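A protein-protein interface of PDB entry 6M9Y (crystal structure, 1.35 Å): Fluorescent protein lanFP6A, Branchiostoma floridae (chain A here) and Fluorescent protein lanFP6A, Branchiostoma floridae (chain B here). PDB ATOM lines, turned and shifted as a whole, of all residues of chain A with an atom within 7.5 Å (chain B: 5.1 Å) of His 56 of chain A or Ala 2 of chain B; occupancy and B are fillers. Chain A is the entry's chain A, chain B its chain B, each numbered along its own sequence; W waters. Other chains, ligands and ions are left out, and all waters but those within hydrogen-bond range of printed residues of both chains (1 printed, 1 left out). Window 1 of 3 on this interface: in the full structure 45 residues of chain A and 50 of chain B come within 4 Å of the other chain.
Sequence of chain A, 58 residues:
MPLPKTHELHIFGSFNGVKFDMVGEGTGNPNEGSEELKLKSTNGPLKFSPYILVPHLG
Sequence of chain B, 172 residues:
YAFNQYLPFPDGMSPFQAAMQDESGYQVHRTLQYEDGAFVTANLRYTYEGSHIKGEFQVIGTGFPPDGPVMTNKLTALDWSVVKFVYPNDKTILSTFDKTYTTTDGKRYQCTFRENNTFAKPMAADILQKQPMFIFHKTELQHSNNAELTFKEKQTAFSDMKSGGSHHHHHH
O of Glu 35 of chain A is in hydrogen-bond range of N of Glu 153 of chain B.
The backbone NH (N) of Tyr 1 of chain B lies within hydrogen-bond range of the backbone carbonyl oxygen (O) of Pro 55 of chain A (2.9 Å).
The backbone carbonyl oxygen (O) of Pro 55 of chain A lies within hydrogen-bond range of the guanidinium group (NH2) of Arg 30 of chain B (2.8 Å).
The backbone NH (N) of Ala 2 of chain B sits at hydrogen-bond distance from the backbone carbonyl oxygen (O) of Leu 57 of chain A (3.5 Å).
OE2 of Glu 35 of chain A lies close to O of Phe 3 of chain B.
OXT of Gly 58 of chain A lies within hydrogen-bond range of NE2 of His 7 of chain A.
O of Tyr 1 of chain B lies within hydrogen-bond range of NH1 of Arg 30 of chain B.
The backbone carbonyl oxygen (O) of Ala 2 of chain B is in hydrogen-bond range of the side-chain hydroxyl (OH) of Tyr 46 of chain B.
N of Arg 30 of chain B is in hydrogen-bond range of O of Ala 42 of chain B (2.9 Å).
The backbone NH of Leu 32 of chain B is in hydrogen-bond range of the backbone carbonyl oxygen of Val 40 of chain B (2.8 Å).
Among the printed residues, pairs that only touch across the chains: His 7 of chain A with Phe 3 of chain B (3.6 Å), Leu 9 of chain A with Phe 57 of chain B (3.4 Å), Ile 11 of chain A with Phe 57 of chain B (3.3 Å), Ile 11 of chain A with Val 59 of chain B (3.99 Å), Phe 15 of chain A with Val 40 of chain B (3.8 Å), His 56 of chain A with Ala 2 of chain B (3.4 Å), His 56 of chain A with Arg 30 of chain B (3.0 Å), His 56 of chain A with Leu 32 of chain B (3.8 Å), His 56 of chain A with Val 40 of chain B (3.95 Å), His 56 of chain A with Phe 57 of chain B (3.2 Å), Leu 57 of chain A with Tyr 1 of chain B (3.5 Å), Leu 57 of chain A with Glu 153 of chain B (3.9 Å), Gly 58 of chain A with Phe 3 of chain B (3.4 Å) and Gly 58 of chain A with Glu 153 of chain B (3.8 Å).
Of the printed residues of chain B, Pro 55 of chain A touches Tyr 1 (2.6 Å) and Arg 30 (2.8 Å).
His 56 of chain A touches five residues of chain B.
Printed residues of chain A within 4 Å of Tyr 1 of chain B: Pro 55 and Leu 57.
Ala 2 of chain B touches two residues of chain A.
The nearest residue of chain B that does not touch His 56 of chain A is Val 59 of chain B (4.05 Å).
The nearest residue of chain A that does not touch Ala 2 of chain B is Gly 58 of chain A (4.1 Å).
Of the 15 printed residues of chain A, 9 touch a printed residue of chain B.
Hydrophobic or aromatic side chains of chain A that line the printed part of chain B: His 7, Leu 9, Ile 11, Phe 15 and His 56.
Of the 14 printed residues of chain B, 9 touch a printed residue of chain A.
Among the printed residues, no Asp or Glu carboxylate lies within 4 Å of a Lys or Arg side-chain nitrogen of the other chain.
Water W1 bridges O of Val 54 of chain A (2.7 Å) and N of Tyr 1 of chain B (2.8 Å).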
ATOM      1  N   HIS A   7      20.044  12.356  -4.200  1.00  0.00           N
ATOM      2  CA  HIS A   7      20.491  12.842  -5.480  1.00  0.00           C
ATOM      3  C   HIS A   7      19.334  13.362  -6.318  1.00  0.00           C
ATOM      4  O   HIS A   7      18.188  12.972  -6.147  1.00  0.00           O
ATOM      5  CB  HIS A   7      21.331  11.797  -6.208  1.00  0.00           C
ATOM      6  CG  HIS A   7      20.628  10.544  -6.593  1.00  0.00           C
ATOM      7  ND1 HIS A   7      20.359   9.554  -5.683  1.00  0.00           N
ATOM      8  CD2 HIS A   7      20.289  10.064  -7.801  1.00  0.00           C
ATOM      9  CE1 HIS A   7      19.829   8.538  -6.313  1.00  0.00           C
ATOM     10  NE2 HIS A   7      19.781   8.833  -7.610  1.00  0.00           N
ATOM     11  N   LEU A   9      18.707  14.323 -10.666  1.00  0.00           N
ATOM     12  CA  LEU A   9      19.236  14.080 -12.002  1.00  0.00           C
ATOM     13  C   LEU A   9      18.486  14.907 -13.039  1.00  0.00           C
ATOM     14  O   LEU A   9      17.251  14.940 -13.046  1.00  0.00           O
ATOM     15  CB  LEU A   9      19.121  12.591 -12.324  1.00  0.00           C
ATOM     16  CG  LEU A   9      19.540  12.185 -13.740  1.00  0.00           C
ATOM     17  CD1 LEU A   9      20.982  12.578 -13.981  1.00  0.00           C
ATOM     18  CD2 LEU A   9      19.365  10.686 -13.942  1.00  0.00           C
ATOM     19  N   ILE A  11      18.679  14.383 -17.014  1.00  0.00           N
ATOM     20  CA  ILE A  11      19.223  13.524 -18.083  1.00  0.00           C
ATOM     21  C   ILE A  11      18.555  13.992 -19.378  1.00  0.00           C
ATOM     22  O   ILE A  11      17.339  14.166 -19.426  1.00  0.00           O
ATOM     23  CB  ILE A  11      19.062  12.021 -17.787  1.00  0.00           C
ATOM     24  CG1 ILE A  11      19.642  11.160 -18.898  1.00  0.00           C
ATOM     25  CG2 ILE A  11      17.614  11.643 -17.517  1.00  0.00           C
ATOM     26  CD1 ILE A  11      19.789   9.693 -18.497  1.00  0.00           C
ATOM     27  N   PHE A  15      17.775  10.971 -29.306  1.00  0.00           N
ATOM     28  CA  PHE A  15      17.803   9.614 -29.923  1.00  0.00           C
ATOM     29  C   PHE A  15      17.339   9.754 -31.373  1.00  0.00           C
ATOM     30  O   PHE A  15      16.284  10.284 -31.620  1.00  0.00           O
ATOM     31  CB  PHE A  15      16.979   8.601 -29.125  1.00  0.00           C
ATOM     32  CG  PHE A  15      17.774   7.983 -28.009  1.00  0.00           C
ATOM     33  CD1 PHE A  15      17.956   8.653 -26.821  1.00  0.00           C
ATOM     34  CD2 PHE A  15      18.368   6.747 -28.156  1.00  0.00           C
ATOM     35  CE1 PHE A  15      18.749   8.121 -25.827  1.00  0.00           C
ATOM     36  CE2 PHE A  15      19.168   6.216 -27.164  1.00  0.00           C
ATOM     37  CZ  PHE A  15      19.349   6.897 -26.001  1.00  0.00           C
ATOM     38  N   GLU A  35      20.260   1.966  -4.630  1.00  0.00           N
ATOM     39  CA  GLU A  35      19.786   3.290  -5.079  1.00  0.00           C
ATOM     40  C   GLU A  35      18.388   3.201  -5.667  1.00  0.00           C
ATOM     41  O   GLU A  35      18.020   2.174  -6.141  1.00  0.00           O
ATOM     42  CB  GLU A  35      20.607   3.860  -6.243  1.00  0.00           C
ATOM     43  CG  GLU A  35      22.080   3.880  -6.013  1.00  0.00           C
ATOM     44  CD  GLU A  35      22.991   4.101  -7.218  1.00  0.00           C
ATOM     45  OE1 GLU A  35      22.663   4.931  -8.029  1.00  0.00           O
ATOM     46  OE2 GLU A  35      24.057   3.435  -7.278  1.00  0.00           O
ATOM     47  N   LEU A  37      15.468   5.902  -7.910  1.00  0.00           N
ATOM     48  CA  LEU A  37      15.280   7.148  -8.651  1.00  0.00           C
ATOM     49  C   LEU A  37      13.886   7.160  -9.241  1.00  0.00           C
ATOM     50  O   LEU A  37      13.381   6.113  -9.668  1.00  0.00           O
ATOM     51  CB  LEU A  37      16.349   7.229  -9.758  1.00  0.00           C
ATOM     52  CG  LEU A  37      16.248   8.431 -10.694  1.00  0.00           C
ATOM     53  CD1 LEU A  37      16.763   9.694 -10.021  1.00  0.00           C
ATOM     54  CD2 LEU A  37      17.042   8.138 -11.974  1.00  0.00           C
ATOM     55  N   LEU A  39      11.938   9.586 -12.265  1.00  0.00           N
ATOM     56  CA  LEU A  39      12.167  10.543 -13.333  1.00  0.00           C
ATOM     57  C   LEU A  39      10.871  10.810 -14.075  1.00  0.00           C
ATOM     58  O   LEU A  39      10.069   9.898 -14.250  1.00  0.00           O
ATOM     59  CB  LEU A  39      13.140   9.972 -14.373  1.00  0.00           C
ATOM     60  CG  LEU A  39      14.624   9.988 -14.105  1.00  0.00           C
ATOM     61  CD1 LEU A  39      15.305   9.353 -15.300  1.00  0.00           C
ATOM     62  CD2 LEU A  39      15.161  11.399 -13.839  1.00  0.00           C
ATOM     63  N   TYR A  51      14.017   1.621 -21.308  1.00  0.00           N
ATOM     64  CA  TYR A  51      15.089   0.694 -20.926  1.00  0.00           C
ATOM     65  C   TYR A  51      16.443   1.107 -21.519  1.00  0.00           C
ATOM     66  O   TYR A  51      17.459   0.771 -20.928  1.00  0.00           O
ATOM     67  CB  TYR A  51      14.758  -0.750 -21.342  1.00  0.00           C
ATOM     68  CG  TYR A  51      13.826  -1.418 -20.354  1.00  0.00           C
ATOM     69  CD1 TYR A  51      14.275  -1.932 -19.147  1.00  0.00           C
ATOM     70  CD2 TYR A  51      12.465  -1.438 -20.575  1.00  0.00           C
ATOM     71  CE1 TYR A  51      13.393  -2.469 -18.207  1.00  0.00           C
ATOM     72  CE2 TYR A  51      11.572  -1.988 -19.665  1.00  0.00           C
ATOM     73  CZ  TYR A  51      12.022  -2.524 -18.460  1.00  0.00           C
ATOM     74  OH  TYR A  51      11.162  -3.052 -17.551  1.00  0.00           O
ATOM     75  N   ILE A  52      16.461   1.851 -22.629  1.00  0.00           N
ATOM     76  CA  ILE A  52      17.746   2.271 -23.235  1.00  0.00           C
ATOM     77  C   ILE A  52      18.480   3.253 -22.295  1.00  0.00           C
ATOM     78  O   ILE A  52      19.680   3.413 -22.392  1.00  0.00           O
ATOM     79  CB  ILE A  52      17.551   2.834 -24.666  1.00  0.00           C
ATOM     80  CG1 ILE A  52      18.791   2.625 -25.538  1.00  0.00           C
ATOM     81  CG2 ILE A  52      17.120   4.296 -24.647  1.00  0.00           C
ATOM     82  CD1 ILE A  52      19.187   1.147 -25.679  1.00  0.00           C
ATOM     83  N   LEU A  53      17.726   3.915 -21.400  1.00  0.00           N
ATOM     84  CA  LEU A  53      18.319   4.858 -20.421  1.00  0.00           C
ATOM     85  C   LEU A  53      18.834   4.179 -19.162  1.00  0.00           C
ATOM     86  O   LEU A  53      19.641   4.781 -18.467  1.00  0.00           O
ATOM     87  CB  LEU A  53      17.330   5.939 -20.021  1.00  0.00           C
ATOM     88  CG  LEU A  53      16.792   6.818 -21.145  1.00  0.00           C
ATOM     89  CD1 LEU A  53      15.808   7.837 -20.595  1.00  0.00           C
ATOM     90  CD2 LEU A  53      17.946   7.508 -21.860  1.00  0.00           C
ATOM     91  N   VAL A  54      18.352   2.973 -18.833  1.00  0.00           N
ATOM     92  CA  VAL A  54      18.619   2.329 -17.557  1.00  0.00           C
ATOM     93  C   VAL A  54      20.097   2.347 -17.166  1.00  0.00           C
ATOM     94  O   VAL A  54      20.421   2.663 -16.013  1.00  0.00           O
ATOM     95  CB  VAL A  54      17.979   0.925 -17.502  1.00  0.00           C
ATOM     96  CG1 VAL A  54      18.587   0.067 -16.391  1.00  0.00           C
ATOM     97  CG2 VAL A  54      16.469   1.072 -17.372  1.00  0.00           C
ATOM     98  N   PRO A  55      21.045   1.995 -18.060  1.00  0.00           N
ATOM     99  CA  PRO A  55      22.439   2.008 -17.633  1.00  0.00           C
ATOM    100  C   PRO A  55      23.023   3.366 -17.279  1.00  0.00           C
ATOM    101  O   PRO A  55      24.085   3.401 -16.702  1.00  0.00           O
ATOM    102  CB  PRO A  55      23.246   1.436 -18.802  1.00  0.00           C
ATOM    103  CG  PRO A  55      22.260   1.244 -19.931  1.00  0.00           C
ATOM    104  CD  PRO A  55      20.869   1.619 -19.470  1.00  0.00           C
ATOM    105  N   HIS A  56      22.304   4.444 -17.645  1.00  0.00           N
ATOM    106  CA  HIS A  56      22.679   5.796 -17.375  1.00  0.00           C
ATOM    107  C   HIS A  56      21.863   6.372 -16.211  1.00  0.00           C
ATOM    108  O   HIS A  56      21.888   7.579 -16.003  1.00  0.00           O
ATOM    109  CB  HIS A  56      22.458   6.645 -18.633  1.00  0.00           C
ATOM    110  CG  HIS A  56      23.102   6.013 -19.819  1.00  0.00           C
ATOM    111  ND1 HIS A  56      22.422   5.421 -20.863  1.00  0.00           N
ATOM    112  CD2 HIS A  56      24.418   5.871 -20.095  1.00  0.00           C
ATOM    113  CE1 HIS A  56      23.324   4.966 -21.738  1.00  0.00           C
ATOM    114  NE2 HIS A  56      24.530   5.215 -21.291  1.00  0.00           N
ATOM    115  N   LEU A  57      21.162   5.532 -15.462  1.00  0.00           N
ATOM    116  CA  LEU A  57      20.399   5.936 -14.272  1.00  0.00           C
ATOM    117  C   LEU A  57      21.091   5.446 -12.992  1.00  0.00           C
ATOM    118  O   LEU A  57      21.816   4.453 -12.987  1.00  0.00           O
ATOM    119  CB  LEU A  57      18.975   5.387 -14.334  1.00  0.00           C
ATOM    120  CG  LEU A  57      18.171   5.762 -15.581  1.00  0.00           C
ATOM    121  CD1 LEU A  57      16.745   5.213 -15.488  1.00  0.00           C
ATOM    122  CD2 LEU A  57      18.168   7.274 -15.826  1.00  0.00           C
ATOM    123  N   GLY A  58      20.826   6.151 -11.902  1.00  0.00           N
ATOM    124  CA  GLY A  58      21.324   5.696 -10.638  1.00  0.00           C
ATOM    125  C   GLY A  58      20.542   6.365  -9.512  1.00  0.00           C
ATOM    126  O   GLY A  58      20.807   6.111  -8.348  1.00  0.00           O
ATOM    127  OXT GLY A  58      19.692   7.133  -9.891  1.00  0.00           O
ATOM    128  N   TYR B   1      24.439   1.816 -14.292  1.00  0.00           N
ATOM    129  CA  TYR B   1      24.826   2.557 -13.060  1.00  0.00           C
ATOM    130  C   TYR B   1      25.280   3.948 -13.510  1.00  0.00           C
ATOM    131  O   TYR B   1      25.513   4.205 -14.667  1.00  0.00           O
ATOM    132  CB  TYR B   1      25.949   1.853 -12.286  1.00  0.00           C
ATOM    133  CG  TYR B   1      27.236   1.694 -13.072  1.00  0.00           C
ATOM    134  CD1 TYR B   1      27.381   0.675 -14.016  1.00  0.00           C
ATOM    135  CD2 TYR B   1      28.271   2.595 -12.998  1.00  0.00           C
ATOM    136  CE1 TYR B   1      28.527   0.535 -14.805  1.00  0.00           C
ATOM    137  CE2 TYR B   1      29.438   2.451 -13.748  1.00  0.00           C
ATOM    138  CZ  TYR B   1      29.565   1.438 -14.665  1.00  0.00           C
ATOM    139  OH  TYR B   1      30.727   1.346 -15.392  1.00  0.00           O
ATOM    140  N   ALA B   2      25.263   4.887 -12.601  1.00  0.00           N
ATOM    141  CA  ALA B   2      25.542   6.239 -12.966  1.00  0.00           C
ATOM    142  C   ALA B   2      25.776   7.129 -11.739  1.00  0.00           C
ATOM    143  O   ALA B   2      26.079   8.294 -11.913  1.00  0.00           O
ATOM    144  CB  ALA B   2      24.377   6.759 -13.772  1.00  0.00           C
ATOM    145  N   PHE B   3      25.555   6.617 -10.529  1.00  0.00           N
ATOM    146  CA  PHE B   3      25.842   7.355  -9.272  1.00  0.00           C
ATOM    147  C   PHE B   3      26.696   6.435  -8.376  1.00  0.00           C
ATOM    148  O   PHE B   3      26.292   6.038  -7.296  1.00  0.00           O
ATOM    149  CB  PHE B   3      24.572   7.855  -8.571  1.00  0.00           C
ATOM    150  CG  PHE B   3      23.901   9.017  -9.249  1.00  0.00           C
ATOM    151  CD1 PHE B   3      24.285  10.321  -8.972  1.00  0.00           C
ATOM    152  CD2 PHE B   3      22.884   8.783 -10.170  1.00  0.00           C
ATOM    153  CE1 PHE B   3      23.649  11.387  -9.593  1.00  0.00           C
ATOM    154  CE2 PHE B   3      22.255   9.844 -10.800  1.00  0.00           C
ATOM    155  CZ  PHE B   3      22.614  11.141 -10.479  1.00  0.00           C
ATOM    156  N   ASN B   4      27.914   6.113  -8.854  1.00  0.00           N
ATOM    157  CA  ASN B   4      28.772   5.179  -8.132  1.00  0.00           C
ATOM    158  C   ASN B   4      29.344   5.739  -6.820  1.00  0.00           C
ATOM    159  O   ASN B   4      30.018   5.022  -6.097  1.00  0.00           O
ATOM    160  CB  ASN B   4      29.880   4.621  -9.030  1.00  0.00           C
ATOM    161  CG  ASN B   4      29.389   3.473  -9.893  1.00  0.00           C
ATOM    162  OD1 ASN B   4      28.211   3.089  -9.841  1.00  0.00           O
ATOM    163  ND2 ASN B   4      30.309   2.918 -10.651  1.00  0.00           N
ATOM    164  N   GLN B   5      28.968   6.967  -6.439  1.00  0.00           N
ATOM    165  CA  GLN B   5      29.192   7.477  -5.102  1.00  0.00           C
ATOM    166  C   GLN B   5      28.432   6.644  -4.044  1.00  0.00           C
ATOM    167  O   GLN B   5      28.786   6.662  -2.855  1.00  0.00           O
ATOM    168  CB  GLN B   5      28.783   8.963  -5.025  1.00  0.00           C
ATOM    169  CG  GLN B   5      29.481   9.849  -6.054  1.00  0.00           C
ATOM    170  CD  GLN B   5      28.693  10.025  -7.338  1.00  0.00           C
ATOM    171  OE1 GLN B   5      27.880   9.159  -7.719  1.00  0.00           O
ATOM    172  NE2 GLN B   5      28.901  11.139  -8.018  1.00  0.00           N
ATOM    173  N   ARG B  30      31.310   7.683 -21.822  1.00  0.00           N
ATOM    174  CA  ARG B  30      30.951   6.307 -22.222  1.00  0.00           C
ATOM    175  C   ARG B  30      30.677   6.233 -23.723  1.00  0.00           C
ATOM    176  O   ARG B  30      30.231   7.195 -24.300  1.00  0.00           O
ATOM    177  CB  ARG B  30      29.604   5.898 -21.608  1.00  0.00           C
ATOM    178  CG  ARG B  30      29.609   5.789 -20.103  1.00  0.00           C
ATOM    179  CD  ARG B  30      28.200   5.613 -19.575  1.00  0.00           C
ATOM    180  NE  ARG B  30      28.358   5.361 -18.175  1.00  0.00           N
ATOM    181  CZ  ARG B  30      27.395   4.904 -17.407  1.00  0.00           C
ATOM    182  NH1 ARG B  30      27.707   4.358 -16.256  1.00  0.00           N
ATOM    183  NH2 ARG B  30      26.145   4.980 -17.802  1.00  0.00           N
ATOM    184  N   LEU B  32      28.800   3.128 -26.251  1.00  0.00           N
ATOM    185  CA  LEU B  32      28.011   1.894 -26.243  1.00  0.00           C
ATOM    186  C   LEU B  32      27.683   1.517 -27.681  1.00  0.00           C
ATOM    187  O   LEU B  32      27.023   2.295 -28.395  1.00  0.00           O
ATOM    188  CB  LEU B  32      26.706   2.118 -25.485  1.00  0.00           C
ATOM    189  CG  LEU B  32      26.755   2.115 -23.970  1.00  0.00           C
ATOM    190  CD1 LEU B  32      27.619   3.181 -23.333  1.00  0.00           C
ATOM    191  CD2 LEU B  32      25.354   2.200 -23.388  1.00  0.00           C
ATOM    192  N   VAL B  40      25.379   4.687 -28.725  1.00  0.00           N
ATOM    193  CA  VAL B  40      25.085   5.713 -27.738  1.00  0.00           C
ATOM    194  C   VAL B  40      26.412   6.204 -27.149  1.00  0.00           C
ATOM    195  O   VAL B  40      27.283   5.401 -26.779  1.00  0.00           O
ATOM    196  CB  VAL B  40      24.144   5.197 -26.631  1.00  0.00           C
ATOM    197  CG1 VAL B  40      24.105   6.125 -25.434  1.00  0.00           C
ATOM    198  CG2 VAL B  40      22.737   4.945 -27.123  1.00  0.00           C
ATOM    199  N   ALA B  42      27.822   9.033 -23.988  1.00  0.00           N
ATOM    200  CA  ALA B  42      27.337   9.779 -22.831  1.00  0.00           C
ATOM    201  C   ALA B  42      28.468  10.453 -22.078  1.00  0.00           C
ATOM    202  O   ALA B  42      29.555   9.933 -22.014  1.00  0.00           O
ATOM    203  CB  ALA B  42      26.548   8.875 -21.914  1.00  0.00           C
ATOM    204  N   LEU B  44      28.710  12.069 -18.168  1.00  0.00           N
ATOM    205  CA  LEU B  44      28.052  12.247 -16.843  1.00  0.00           C
ATOM    206  C   LEU B  44      28.925  13.209 -16.046  1.00  0.00           C
ATOM    207  O   LEU B  44      30.122  12.995 -15.903  1.00  0.00           O
ATOM    208  CB  LEU B  44      27.878  10.935 -16.073  1.00  0.00           C
ATOM    209  CG  LEU B  44      27.495   9.690 -16.859  1.00  0.00           C
ATOM    210  CD1 LEU B  44      27.322   8.488 -15.936  1.00  0.00           C
ATOM    211  CD2 LEU B  44      26.258   9.853 -17.749  1.00  0.00           C
ATOM    212  N   TYR B  46      28.870  15.734 -12.353  1.00  0.00           N
ATOM    213  CA  TYR B  46      28.267  15.861 -11.016  1.00  0.00           C
ATOM    214  C   TYR B  46      28.683  17.172 -10.363  1.00  0.00           C
ATOM    215  O   TYR B  46      29.832  17.594 -10.468  1.00  0.00           O
ATOM    216  CB  TYR B  46      28.711  14.720 -10.080  1.00  0.00           C
ATOM    217  CG  TYR B  46      28.559  13.354 -10.717  1.00  0.00           C
ATOM    218  CD1 TYR B  46      27.352  12.691 -10.667  1.00  0.00           C
ATOM    219  CD2 TYR B  46      29.625  12.741 -11.341  1.00  0.00           C
ATOM    220  CE1 TYR B  46      27.174  11.447 -11.246  1.00  0.00           C
ATOM    221  CE2 TYR B  46      29.466  11.501 -11.944  1.00  0.00           C
ATOM    222  CZ  TYR B  46      28.239  10.863 -11.911  1.00  0.00           C
ATOM    223  OH  TYR B  46      28.144   9.628 -12.503  1.00  0.00           O
ATOM    224  N   PHE B  57      23.510  14.616 -17.032  1.00  0.00           N
ATOM    225  CA  PHE B  57      23.884  13.514 -17.911  1.00  0.00           C
ATOM    226  C   PHE B  57      23.377  13.777 -19.339  1.00  0.00           C
ATOM    227  O   PHE B  57      22.171  13.901 -19.588  1.00  0.00           O
ATOM    228  CB  PHE B  57      23.273  12.196 -17.442  1.00  0.00           C
ATOM    229  CG  PHE B  57      23.696  11.648 -16.102  1.00  0.00           C
ATOM    230  CD1 PHE B  57      24.572  12.319 -15.263  1.00  0.00           C
ATOM    231  CD2 PHE B  57      23.096  10.487 -15.631  1.00  0.00           C
ATOM    232  CE1 PHE B  57      24.906  11.810 -14.021  1.00  0.00           C
ATOM    233  CE2 PHE B  57      23.413  10.001 -14.382  1.00  0.00           C
ATOM    234  CZ  PHE B  57      24.334  10.660 -13.581  1.00  0.00           C
ATOM    235  N   VAL B  59      23.132  12.176 -22.973  1.00  0.00           N
ATOM    236  CA  VAL B  59      23.085  10.860 -23.599  1.00  0.00           C
ATOM    237  C   VAL B  59      22.580  11.050 -25.029  1.00  0.00           C
ATOM    238  O   VAL B  59      21.459  11.531 -25.253  1.00  0.00           O
ATOM    239  CB  VAL B  59      22.159   9.902 -22.819  1.00  0.00           C
ATOM    240  CG1 VAL B  59      22.141   8.520 -23.451  1.00  0.00           C
ATOM    241  CG2 VAL B  59      22.561   9.776 -21.362  1.00  0.00           C
ATOM    242  N   GLU B 153      18.227  -0.110  -8.071  1.00  0.00           N
ATOM    243  CA  GLU B 153      19.495  -0.791  -8.370  1.00  0.00           C
ATOM    244  C   GLU B 153      20.177  -1.311  -7.110  1.00  0.00           C
ATOM    245  O   GLU B 153      20.035  -0.721  -6.029  1.00  0.00           O
ATOM    246  CB  GLU B 153      20.360   0.227  -9.101  1.00  0.00           C
ATOM    247  CG  GLU B 153      21.801   0.223  -8.704  1.00  0.00           C
ATOM    248  CD  GLU B 153      22.529   0.929  -9.810  1.00  0.00           C
ATOM    249  OE1 GLU B 153      22.335   2.159  -9.882  1.00  0.00           O
ATOM    250  OE2 GLU B 153      23.231   0.244 -10.583  1.00  0.00           O
HETATM  251  O   HOH W   1      21.734   0.949 -14.448  1.00  0.00           O
